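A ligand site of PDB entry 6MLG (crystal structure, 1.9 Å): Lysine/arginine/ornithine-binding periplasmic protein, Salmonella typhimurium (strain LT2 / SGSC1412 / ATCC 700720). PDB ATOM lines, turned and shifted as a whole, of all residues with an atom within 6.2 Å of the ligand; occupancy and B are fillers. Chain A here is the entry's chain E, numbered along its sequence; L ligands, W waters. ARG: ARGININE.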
ATOM      1  N   THR A  10      -5.490 -24.755  -7.745  1.00  0.00           N
ATOM      2  CA  THR A  10      -6.780 -24.436  -8.335  1.00  0.00           C
ATOM      3  C   THR A  10      -7.890 -24.801  -7.343  1.00  0.00           C
ATOM      4  O   THR A  10      -7.722 -25.692  -6.504  1.00  0.00           O
ATOM      5  CB  THR A  10      -6.985 -25.168  -9.696  1.00  0.00           C
ATOM      6  OG1 THR A  10      -8.145 -24.652 -10.370  1.00  0.00           O
ATOM      7  CG2 THR A  10      -7.156 -26.671  -9.492  1.00  0.00           C
ATOM      8  N   ASP A  11      -9.010 -24.097  -7.441  1.00  0.00           N
ATOM      9  CA  ASP A  11     -10.195 -24.486  -6.697  1.00  0.00           C
ATOM     10  C   ASP A  11     -11.126 -25.272  -7.620  1.00  0.00           C
ATOM     11  O   ASP A  11     -11.582 -24.757  -8.655  1.00  0.00           O
ATOM     12  CB  ASP A  11     -10.945 -23.288  -6.139  1.00  0.00           C
ATOM     13  CG  ASP A  11     -12.392 -23.622  -5.840  1.00  0.00           C
ATOM     14  OD1 ASP A  11     -12.662 -24.138  -4.744  1.00  0.00           O
ATOM     15  OD2 ASP A  11     -13.246 -23.417  -6.730  1.00  0.00           O
ATOM     16  N   THR A  12     -11.423 -26.492  -7.228  1.00  0.00           N
ATOM     17  CA  THR A  12     -12.126 -27.429  -8.100  1.00  0.00           C
ATOM     18  C   THR A  12     -13.649 -27.437  -7.921  1.00  0.00           C
ATOM     19  O   THR A  12     -14.291 -28.477  -8.062  1.00  0.00           O
ATOM     20  CB  THR A  12     -11.604 -28.852  -7.889  1.00  0.00           C
ATOM     21  OG1 THR A  12     -11.727 -29.205  -6.498  1.00  0.00           O
ATOM     22  CG2 THR A  12     -10.162 -28.938  -8.309  1.00  0.00           C
ATOM     23  N   THR A  13     -14.234 -26.273  -7.629  1.00  0.00           N
ATOM     24  CA  THR A  13     -15.682 -26.185  -7.527  1.00  0.00           C
ATOM     25  C   THR A  13     -16.224 -25.175  -8.544  1.00  0.00           C
ATOM     26  O   THR A  13     -17.189 -24.464  -8.272  1.00  0.00           O
ATOM     27  CB  THR A  13     -16.127 -25.789  -6.111  1.00  0.00           C
ATOM     28  OG1 THR A  13     -15.639 -24.473  -5.793  1.00  0.00           O
ATOM     29  CG2 THR A  13     -15.585 -26.766  -5.086  1.00  0.00           C
ATOM     30  N   TYR A  14     -15.614 -25.133  -9.727  1.00  0.00           N
ATOM     31  CA  TYR A  14     -15.954 -24.105 -10.699  1.00  0.00           C
ATOM     32  C   TYR A  14     -16.006 -24.670 -12.118  1.00  0.00           C
ATOM     33  O   TYR A  14     -15.293 -24.201 -13.014  1.00  0.00           O
ATOM     34  CB  TYR A  14     -14.932 -22.957 -10.572  1.00  0.00           C
ATOM     35  CG  TYR A  14     -15.493 -21.553 -10.556  1.00  0.00           C
ATOM     36  CD1 TYR A  14     -16.321 -21.129  -9.509  1.00  0.00           C
ATOM     37  CD2 TYR A  14     -15.102 -20.616 -11.508  1.00  0.00           C
ATOM     38  CE1 TYR A  14     -16.796 -19.809  -9.461  1.00  0.00           C
ATOM     39  CE2 TYR A  14     -15.574 -19.295 -11.451  1.00  0.00           C
ATOM     40  CZ  TYR A  14     -16.423 -18.913 -10.436  1.00  0.00           C
ATOM     41  OH  TYR A  14     -16.887 -17.604 -10.380  1.00  0.00           O
ATOM     42  N   PHE A  17     -14.596 -24.889 -15.691  1.00  0.00           N
ATOM     43  CA  PHE A  17     -13.196 -24.496 -15.746  1.00  0.00           C
ATOM     44  C   PHE A  17     -12.339 -25.405 -14.868  1.00  0.00           C
ATOM     45  O   PHE A  17     -11.275 -25.870 -15.293  1.00  0.00           O
ATOM     46  CB  PHE A  17     -13.027 -23.029 -15.330  1.00  0.00           C
ATOM     47  CG  PHE A  17     -13.785 -22.077 -16.203  1.00  0.00           C
ATOM     48  CD1 PHE A  17     -13.306 -21.722 -17.463  1.00  0.00           C
ATOM     49  CD2 PHE A  17     -14.994 -21.541 -15.777  1.00  0.00           C
ATOM     50  CE1 PHE A  17     -14.017 -20.832 -18.273  1.00  0.00           C
ATOM     51  CE2 PHE A  17     -15.709 -20.661 -16.595  1.00  0.00           C
ATOM     52  CZ  PHE A  17     -15.217 -20.308 -17.849  1.00  0.00           C
ATOM     53  N   SER A  18     -12.811 -25.666 -13.661  1.00  0.00           N
ATOM     54  CA  SER A  18     -12.035 -26.494 -12.763  1.00  0.00           C
ATOM     55  C   SER A  18     -12.955 -27.221 -11.804  1.00  0.00           C
ATOM     56  O   SER A  18     -13.632 -26.585 -10.988  1.00  0.00           O
ATOM     57  CB  SER A  18     -11.031 -25.653 -11.986  1.00  0.00           C
ATOM     58  OG  SER A  18     -10.182 -26.481 -11.198  1.00  0.00           O
ATOM     59  N   ASP A  30      -9.640 -25.002 -17.585  1.00  0.00           N
ATOM     60  CA  ASP A  30      -8.420 -24.578 -16.889  1.00  0.00           C
ATOM     61  C   ASP A  30      -7.384 -25.707 -16.851  1.00  0.00           C
ATOM     62  O   ASP A  30      -6.196 -25.492 -17.124  1.00  0.00           O
ATOM     63  CB  ASP A  30      -8.729 -24.143 -15.450  1.00  0.00           C
ATOM     64  CG  ASP A  30      -9.123 -22.683 -15.326  1.00  0.00           C
ATOM     65  OD1 ASP A  30      -9.048 -21.925 -16.312  1.00  0.00           O
ATOM     66  OD2 ASP A  30      -9.503 -22.286 -14.209  1.00  0.00           O
ATOM     67  N   PHE A  52     -10.504 -21.372  -2.872  1.00  0.00           N
ATOM     68  CA  PHE A  52     -10.109 -20.239  -3.694  1.00  0.00           C
ATOM     69  C   PHE A  52      -9.361 -19.176  -2.881  1.00  0.00           C
ATOM     70  O   PHE A  52      -8.326 -18.668  -3.318  1.00  0.00           O
ATOM     71  CB  PHE A  52     -11.339 -19.625  -4.363  1.00  0.00           C
ATOM     72  CG  PHE A  52     -11.004 -18.559  -5.350  1.00  0.00           C
ATOM     73  CD1 PHE A  52     -10.501 -18.898  -6.600  1.00  0.00           C
ATOM     74  CD2 PHE A  52     -11.144 -17.210  -5.028  1.00  0.00           C
ATOM     75  CE1 PHE A  52     -10.152 -17.925  -7.509  1.00  0.00           C
ATOM     76  CE2 PHE A  52     -10.797 -16.228  -5.948  1.00  0.00           C
ATOM     77  CZ  PHE A  52     -10.307 -16.585  -7.192  1.00  0.00           C
ATOM     78  N   LEU A  55      -5.594 -19.545  -2.351  1.00  0.00           N
ATOM     79  CA  LEU A  55      -4.687 -19.660  -3.496  1.00  0.00           C
ATOM     80  C   LEU A  55      -3.583 -18.621  -3.494  1.00  0.00           C
ATOM     81  O   LEU A  55      -2.418 -18.964  -3.603  1.00  0.00           O
ATOM     82  CB  LEU A  55      -5.456 -19.573  -4.830  1.00  0.00           C
ATOM     83  CG  LEU A  55      -6.325 -20.794  -5.162  1.00  0.00           C
ATOM     84  CD1 LEU A  55      -7.251 -20.497  -6.344  1.00  0.00           C
ATOM     85  CD2 LEU A  55      -5.457 -22.013  -5.441  1.00  0.00           C
ATOM     86  N   ILE A  68      -4.093 -21.582 -11.617  1.00  0.00           N
ATOM     87  CA  ILE A  68      -4.989 -21.554 -12.763  1.00  0.00           C
ATOM     88  C   ILE A  68      -6.364 -21.939 -12.240  1.00  0.00           C
ATOM     89  O   ILE A  68      -6.620 -23.103 -11.962  1.00  0.00           O
ATOM     90  CB  ILE A  68      -4.511 -22.489 -13.898  1.00  0.00           C
ATOM     91  CG1 ILE A  68      -3.096 -22.075 -14.320  1.00  0.00           C
ATOM     92  CG2 ILE A  68      -5.460 -22.406 -15.084  1.00  0.00           C
ATOM     93  CD1 ILE A  68      -2.484 -22.945 -15.391  1.00  0.00           C
ATOM     94  N   SER A  69      -7.222 -20.935 -12.063  1.00  0.00           N
ATOM     95  CA  SER A  69      -8.447 -21.117 -11.302  1.00  0.00           C
ATOM     96  C   SER A  69      -9.438 -19.986 -11.600  1.00  0.00           C
ATOM     97  O   SER A  69     -10.018 -19.403 -10.675  1.00  0.00           O
ATOM     98  CB  SER A  69      -8.103 -21.175  -9.802  1.00  0.00           C
ATOM     99  OG  SER A  69      -9.174 -21.650  -9.004  1.00  0.00           O
ATOM    100  N   SER A  70      -9.612 -19.692 -12.894  1.00  0.00           N
ATOM    101  CA  SER A  70     -10.414 -18.542 -13.355  1.00  0.00           C
ATOM    102  C   SER A  70     -10.071 -17.280 -12.577  1.00  0.00           C
ATOM    103  O   SER A  70     -10.954 -16.534 -12.178  1.00  0.00           O
ATOM    104  CB  SER A  70     -11.920 -18.832 -13.241  1.00  0.00           C
ATOM    105  OG  SER A  70     -12.292 -19.963 -14.010  1.00  0.00           O
ATOM    106  N   LEU A  71      -8.782 -17.056 -12.344  1.00  0.00           N
ATOM    107  CA  LEU A  71      -8.366 -15.928 -11.538  1.00  0.00           C
ATOM    108  C   LEU A  71      -8.284 -14.652 -12.370  1.00  0.00           C
ATOM    109  O   LEU A  71      -7.425 -14.515 -13.223  1.00  0.00           O
ATOM    110  CB  LEU A  71      -7.015 -16.227 -10.876  1.00  0.00           C
ATOM    111  CG  LEU A  71      -6.408 -15.152  -9.972  1.00  0.00           C
ATOM    112  CD1 LEU A  71      -7.294 -14.898  -8.772  1.00  0.00           C
ATOM    113  CD2 LEU A  71      -5.028 -15.597  -9.541  1.00  0.00           C
ATOM    114  N   SER A  72      -9.213 -13.725 -12.119  1.00  0.00           N
ATOM    115  CA  SER A  72      -9.284 -12.482 -12.896  1.00  0.00           C
ATOM    116  C   SER A  72      -8.036 -11.624 -12.748  1.00  0.00           C
ATOM    117  O   SER A  72      -7.505 -11.462 -11.640  1.00  0.00           O
ATOM    118  CB  SER A  72     -10.513 -11.667 -12.488  1.00  0.00           C
ATOM    119  OG  SER A  72     -11.692 -12.338 -12.869  1.00  0.00           O
ATOM    120  N   ILE A  73      -7.587 -11.088 -13.876  1.00  0.00           N
ATOM    121  CA  ILE A  73      -6.494 -10.126 -13.917  1.00  0.00           C
ATOM    122  C   ILE A  73      -7.026  -8.750 -13.525  1.00  0.00           C
ATOM    123  O   ILE A  73      -7.542  -8.005 -14.358  1.00  0.00           O
ATOM    124  CB  ILE A  73      -5.855 -10.064 -15.324  1.00  0.00           C
ATOM    125  CG1 ILE A  73      -5.530 -11.487 -15.820  1.00  0.00           C
ATOM    126  CG2 ILE A  73      -4.619  -9.145 -15.326  1.00  0.00           C
ATOM    127  CD1 ILE A  73      -5.253 -11.565 -17.333  1.00  0.00           C
ATOM    128  N   THR A  74      -6.928  -8.432 -12.239  1.00  0.00           N
ATOM    129  CA  THR A  74      -7.394  -7.154 -11.734  1.00  0.00           C
ATOM    130  C   THR A  74      -6.234  -6.280 -11.269  1.00  0.00           C
ATOM    131  O   THR A  74      -5.143  -6.765 -10.999  1.00  0.00           O
ATOM    132  CB  THR A  74      -8.363  -7.322 -10.563  1.00  0.00           C
ATOM    133  OG1 THR A  74      -7.622  -7.808  -9.439  1.00  0.00           O
ATOM    134  CG2 THR A  74      -9.481  -8.319 -10.904  1.00  0.00           C
ATOM    135  N   ALA A  90     -13.988 -13.251 -18.523  1.00  0.00           N
ATOM    136  CA  ALA A  90     -14.850 -13.659 -17.433  1.00  0.00           C
ATOM    137  C   ALA A  90     -15.666 -12.501 -16.880  1.00  0.00           C
ATOM    138  O   ALA A  90     -15.175 -11.699 -16.092  1.00  0.00           O
ATOM    139  CB  ALA A  90     -14.022 -14.294 -16.293  1.00  0.00           C
ATOM    140  N   SER A  92     -19.158 -11.259 -14.682  1.00  0.00           N
ATOM    141  CA  SER A  92     -19.932 -11.728 -13.543  1.00  0.00           C
ATOM    142  C   SER A  92     -21.416 -11.540 -13.830  1.00  0.00           C
ATOM    143  O   SER A  92     -21.803 -10.606 -14.543  1.00  0.00           O
ATOM    144  CB  SER A  92     -19.526 -10.979 -12.274  1.00  0.00           C
ATOM    145  OG  SER A  92     -18.169 -11.268 -11.934  1.00  0.00           O
ATOM    146  N   LEU A 117     -18.422 -16.232  -3.530  1.00  0.00           N
ATOM    147  CA  LEU A 117     -17.246 -17.008  -3.169  1.00  0.00           C
ATOM    148  C   LEU A 117     -16.276 -16.162  -2.338  1.00  0.00           C
ATOM    149  O   LEU A 117     -15.947 -15.040  -2.723  1.00  0.00           O
ATOM    150  CB  LEU A 117     -16.570 -17.549  -4.429  1.00  0.00           C
ATOM    151  CG  LEU A 117     -15.249 -18.290  -4.185  1.00  0.00           C
ATOM    152  CD1 LEU A 117     -15.530 -19.565  -3.399  1.00  0.00           C
ATOM    153  CD2 LEU A 117     -14.573 -18.605  -5.518  1.00  0.00           C
ATOM    154  N   GLY A 119     -13.051 -14.487  -0.995  1.00  0.00           N
ATOM    155  CA  GLY A 119     -11.790 -14.149  -1.634  1.00  0.00           C
ATOM    156  C   GLY A 119     -11.920 -13.821  -3.116  1.00  0.00           C
ATOM    157  O   GLY A 119     -10.916 -13.579  -3.774  1.00  0.00           O
ATOM    158  N   SER A 120     -13.150 -13.815  -3.645  1.00  0.00           N
ATOM    159  CA  SER A 120     -13.348 -13.568  -5.075  1.00  0.00           C
ATOM    160  C   SER A 120     -13.582 -12.084  -5.381  1.00  0.00           C
ATOM    161  O   SER A 120     -13.880 -11.284  -4.488  1.00  0.00           O
ATOM    162  CB  SER A 120     -14.539 -14.395  -5.607  1.00  0.00           C
ATOM    163  OG  SER A 120     -15.767 -13.887  -5.120  1.00  0.00           O
ATOM    164  N   THR A 121     -13.432 -11.728  -6.655  1.00  0.00           N
ATOM    165  CA  THR A 121     -13.836 -10.410  -7.121  1.00  0.00           C
ATOM    166  C   THR A 121     -15.315 -10.159  -6.810  1.00  0.00           C
ATOM    167  O   THR A 121     -15.705  -9.029  -6.488  1.00  0.00           O
ATOM    168  CB  THR A 121     -13.609 -10.220  -8.630  1.00  0.00           C
ATOM    169  OG1 THR A 121     -14.313 -11.235  -9.346  1.00  0.00           O
ATOM    170  CG2 THR A 121     -12.125 -10.273  -8.981  1.00  0.00           C
ATOM    171  N   GLN A 122     -16.133 -11.205  -6.889  1.00  0.00           N
ATOM    172  CA  GLN A 122     -17.565 -11.043  -6.628  1.00  0.00           C
ATOM    173  C   GLN A 122     -17.817 -10.728  -5.156  1.00  0.00           C
ATOM    174  O   GLN A 122     -18.724  -9.961  -4.845  1.00  0.00           O
ATOM    175  CB  GLN A 122     -18.341 -12.306  -7.043  1.00  0.00           C
ATOM    176  CG  GLN A 122     -18.416 -12.550  -8.546  1.00  0.00           C
ATOM    177  CD  GLN A 122     -17.227 -13.339  -9.102  1.00  0.00           C
ATOM    178  OE1 GLN A 122     -16.398 -13.860  -8.345  1.00  0.00           O
ATOM    179  NE2 GLN A 122     -17.134 -13.421 -10.412  1.00  0.00           N
ATOM    180  N   GLN A 143     -17.683 -22.759  -4.194  1.00  0.00           N
ATOM    181  CA  GLN A 143     -18.863 -22.432  -4.981  1.00  0.00           C
ATOM    182  C   GLN A 143     -19.921 -23.542  -4.918  1.00  0.00           C
ATOM    183  O   GLN A 143     -21.107 -23.279  -5.145  1.00  0.00           O
ATOM    184  CB  GLN A 143     -18.471 -22.155  -6.449  1.00  0.00           C
ATOM    185  CG  GLN A 143     -19.659 -21.784  -7.365  1.00  0.00           C
ATOM    186  CD  GLN A 143     -20.138 -20.331  -7.201  1.00  0.00           C
ATOM    187  OE1 GLN A 143     -19.374 -19.458  -6.790  1.00  0.00           O
ATOM    188  NE2 GLN A 143     -21.422 -20.093  -7.509  1.00  0.00           N
ATOM    189  N   ASP A 161     -18.794 -15.970 -11.786  1.00  0.00           N
ATOM    190  CA  ASP A 161     -18.497 -15.832 -13.208  1.00  0.00           C
ATOM    191  C   ASP A 161     -19.659 -16.362 -14.043  1.00  0.00           C
ATOM    192  O   ASP A 161     -20.196 -17.448 -13.759  1.00  0.00           O
ATOM    193  CB  ASP A 161     -17.208 -16.573 -13.591  1.00  0.00           C
ATOM    194  CG  ASP A 161     -15.947 -15.886 -13.070  1.00  0.00           C
ATOM    195  OD1 ASP A 161     -16.028 -14.748 -12.570  1.00  0.00           O
ATOM    196  OD2 ASP A 161     -14.847 -16.493 -13.176  1.00  0.00           O
ATOM    197  N   THR A 195      -9.099 -13.717 -17.324  1.00  0.00           N
ATOM    198  CA  THR A 195      -8.374 -14.488 -16.328  1.00  0.00           C
ATOM    199  C   THR A 195      -6.987 -14.800 -16.878  1.00  0.00           C
ATOM    200  O   THR A 195      -6.764 -14.707 -18.090  1.00  0.00           O
ATOM    201  CB  THR A 195      -9.093 -15.808 -15.992  1.00  0.00           C
ATOM    202  OG1 THR A 195      -9.161 -16.630 -17.159  1.00  0.00           O
ATOM    203  CG2 THR A 195     -10.519 -15.538 -15.499  1.00  0.00           C
HETATM  204  N   ARG L   1     -13.069 -14.679 -11.405  1.00  0.00           N
HETATM  205  CA  ARG L   1     -13.298 -14.570  -9.965  1.00  0.00           C
HETATM  206  C   ARG L   1     -12.023 -14.077  -9.284  1.00  0.00           C
HETATM  207  O   ARG L   1     -12.028 -13.752  -8.089  1.00  0.00           O
HETATM  208  CB  ARG L   1     -13.765 -15.919  -9.364  1.00  0.00           C
HETATM  209  CG  ARG L   1     -12.880 -17.120  -9.703  1.00  0.00           C
HETATM  210  CD  ARG L   1     -13.291 -18.404  -8.946  1.00  0.00           C
HETATM  211  NE  ARG L   1     -12.561 -19.583  -9.413  1.00  0.00           N
HETATM  212  CZ  ARG L   1     -12.638 -20.803  -8.874  1.00  0.00           C
HETATM  213  NH1 ARG L   1     -11.919 -21.811  -9.374  1.00  0.00           N
HETATM  214  NH2 ARG L   1     -13.412 -21.029  -7.820  1.00  0.00           N
HETATM  215  OXT ARG L   1     -10.971 -13.966  -9.925  1.00  0.00           O
HETATM  216  O   HOH W   1      -9.826 -12.890  -7.104  1.00  0.00           O
HETATM  217  O   HOH W   2      -8.608 -11.668  -9.188  1.00  0.00           O
HETATM  218  O   HOH W   3     -13.806 -11.333 -11.734  1.00  0.00           O
HETATM  219  O   HOH W   4     -11.571 -22.157 -12.291  1.00  0.00           O
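OD2 of Asp 11 is in hydrogen-bond range of OG1 of Thr 13 (2.8 Å).
O of Asp 11 sits at hydrogen-bond distance from OG of Ser 18, at 3.4 Å.
OG of Ser 69 sits at hydrogen-bond distance from OG1 of Thr 10.
The backbone NH (N) of Ser 69 sits close to the side-chain carboxylate (OD2) of Asp 30 (3.4 Å).
The side-chain hydroxyl of Tyr 14 is in hydrogen-bond range of the backbone NH of Asp 161, 2.9 Å away.
N of Gln 122 sits close to OG of Ser 120 (3.2 Å).
The side-chain hydroxyl of Ser 120 sits at hydrogen-bond distance from the backbone carbonyl oxygen of Leu 117 (2.7 Å).
OG of Ser 92 sits at hydrogen-bond distance from NE2 of Gln 122 (2.8 Å).
Water W4 lies within hydrogen-bond range of the side-chain carboxylate of Asp 30, the side-chain hydroxyl of Ser 70 and a nitrogen (NH1) of the ligand.
Water W2 lies within hydrogen-bond range of O of Ser 72 and OXT of the ligand.
Water W3 lies within hydrogen-bond range of the side-chain hydroxyl of Thr 121, the side-chain hydroxyl of Ser 72 and a nitrogen (N) of the ligand.
Tyr 14 touches the ligand (CD1 to NH2, 3.4 Å).
Phe 52 touches the ligand.
Leu 71 touches the ligand (CA to OXT, 3.6 Å).
Leu 117 touches the ligand (CD2 to NH2, 3.5 Å).
Ser 120 touches the ligand (CA to O, 3.3 Å).
Gln 122 touches the ligand.
Hydrophobic or aromatic side chains within 4 Å of the ligand: Tyr 14, Phe 52, Leu 71 and Leu 117.
Along chain A the residues within 4 Å of the ligand span positions 11 to 161.
A nitrogen (NH1) of the ligand is in hydrogen-bond range of the backbone carbonyl oxygen (O) of Asp 11 (3.1 Å).
OD2 of Asp 11 is in salt-bridge range of NH2 of the ligand.
O of Ser 69 lies within hydrogen-bond range of NE of the ligand (2.8 Å).
NH1 of the ligand sits at hydrogen-bond distance from OG of Ser 69, at 2.8 Å.
An oxygen (OXT) of the ligand lies within hydrogen-bond range of the backbone NH (N) of Ser 72, 2.8 Å away.
N of the ligand sits at hydrogen-bond distance from OG of Ser 72 (3.1 Å).
An oxygen (O) of the ligand lies within hydrogen-bond range of the backbone NH (N) of Thr 121, 2.9 Å away.
The backbone carbonyl oxygen (O) of Ser 70 sits at hydrogen-bond distance from a nitrogen (N) of the ligand, at 2.9 Å.
OD2 of Asp 161 lies within salt-bridge range of N of the ligand (3.1 Å).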
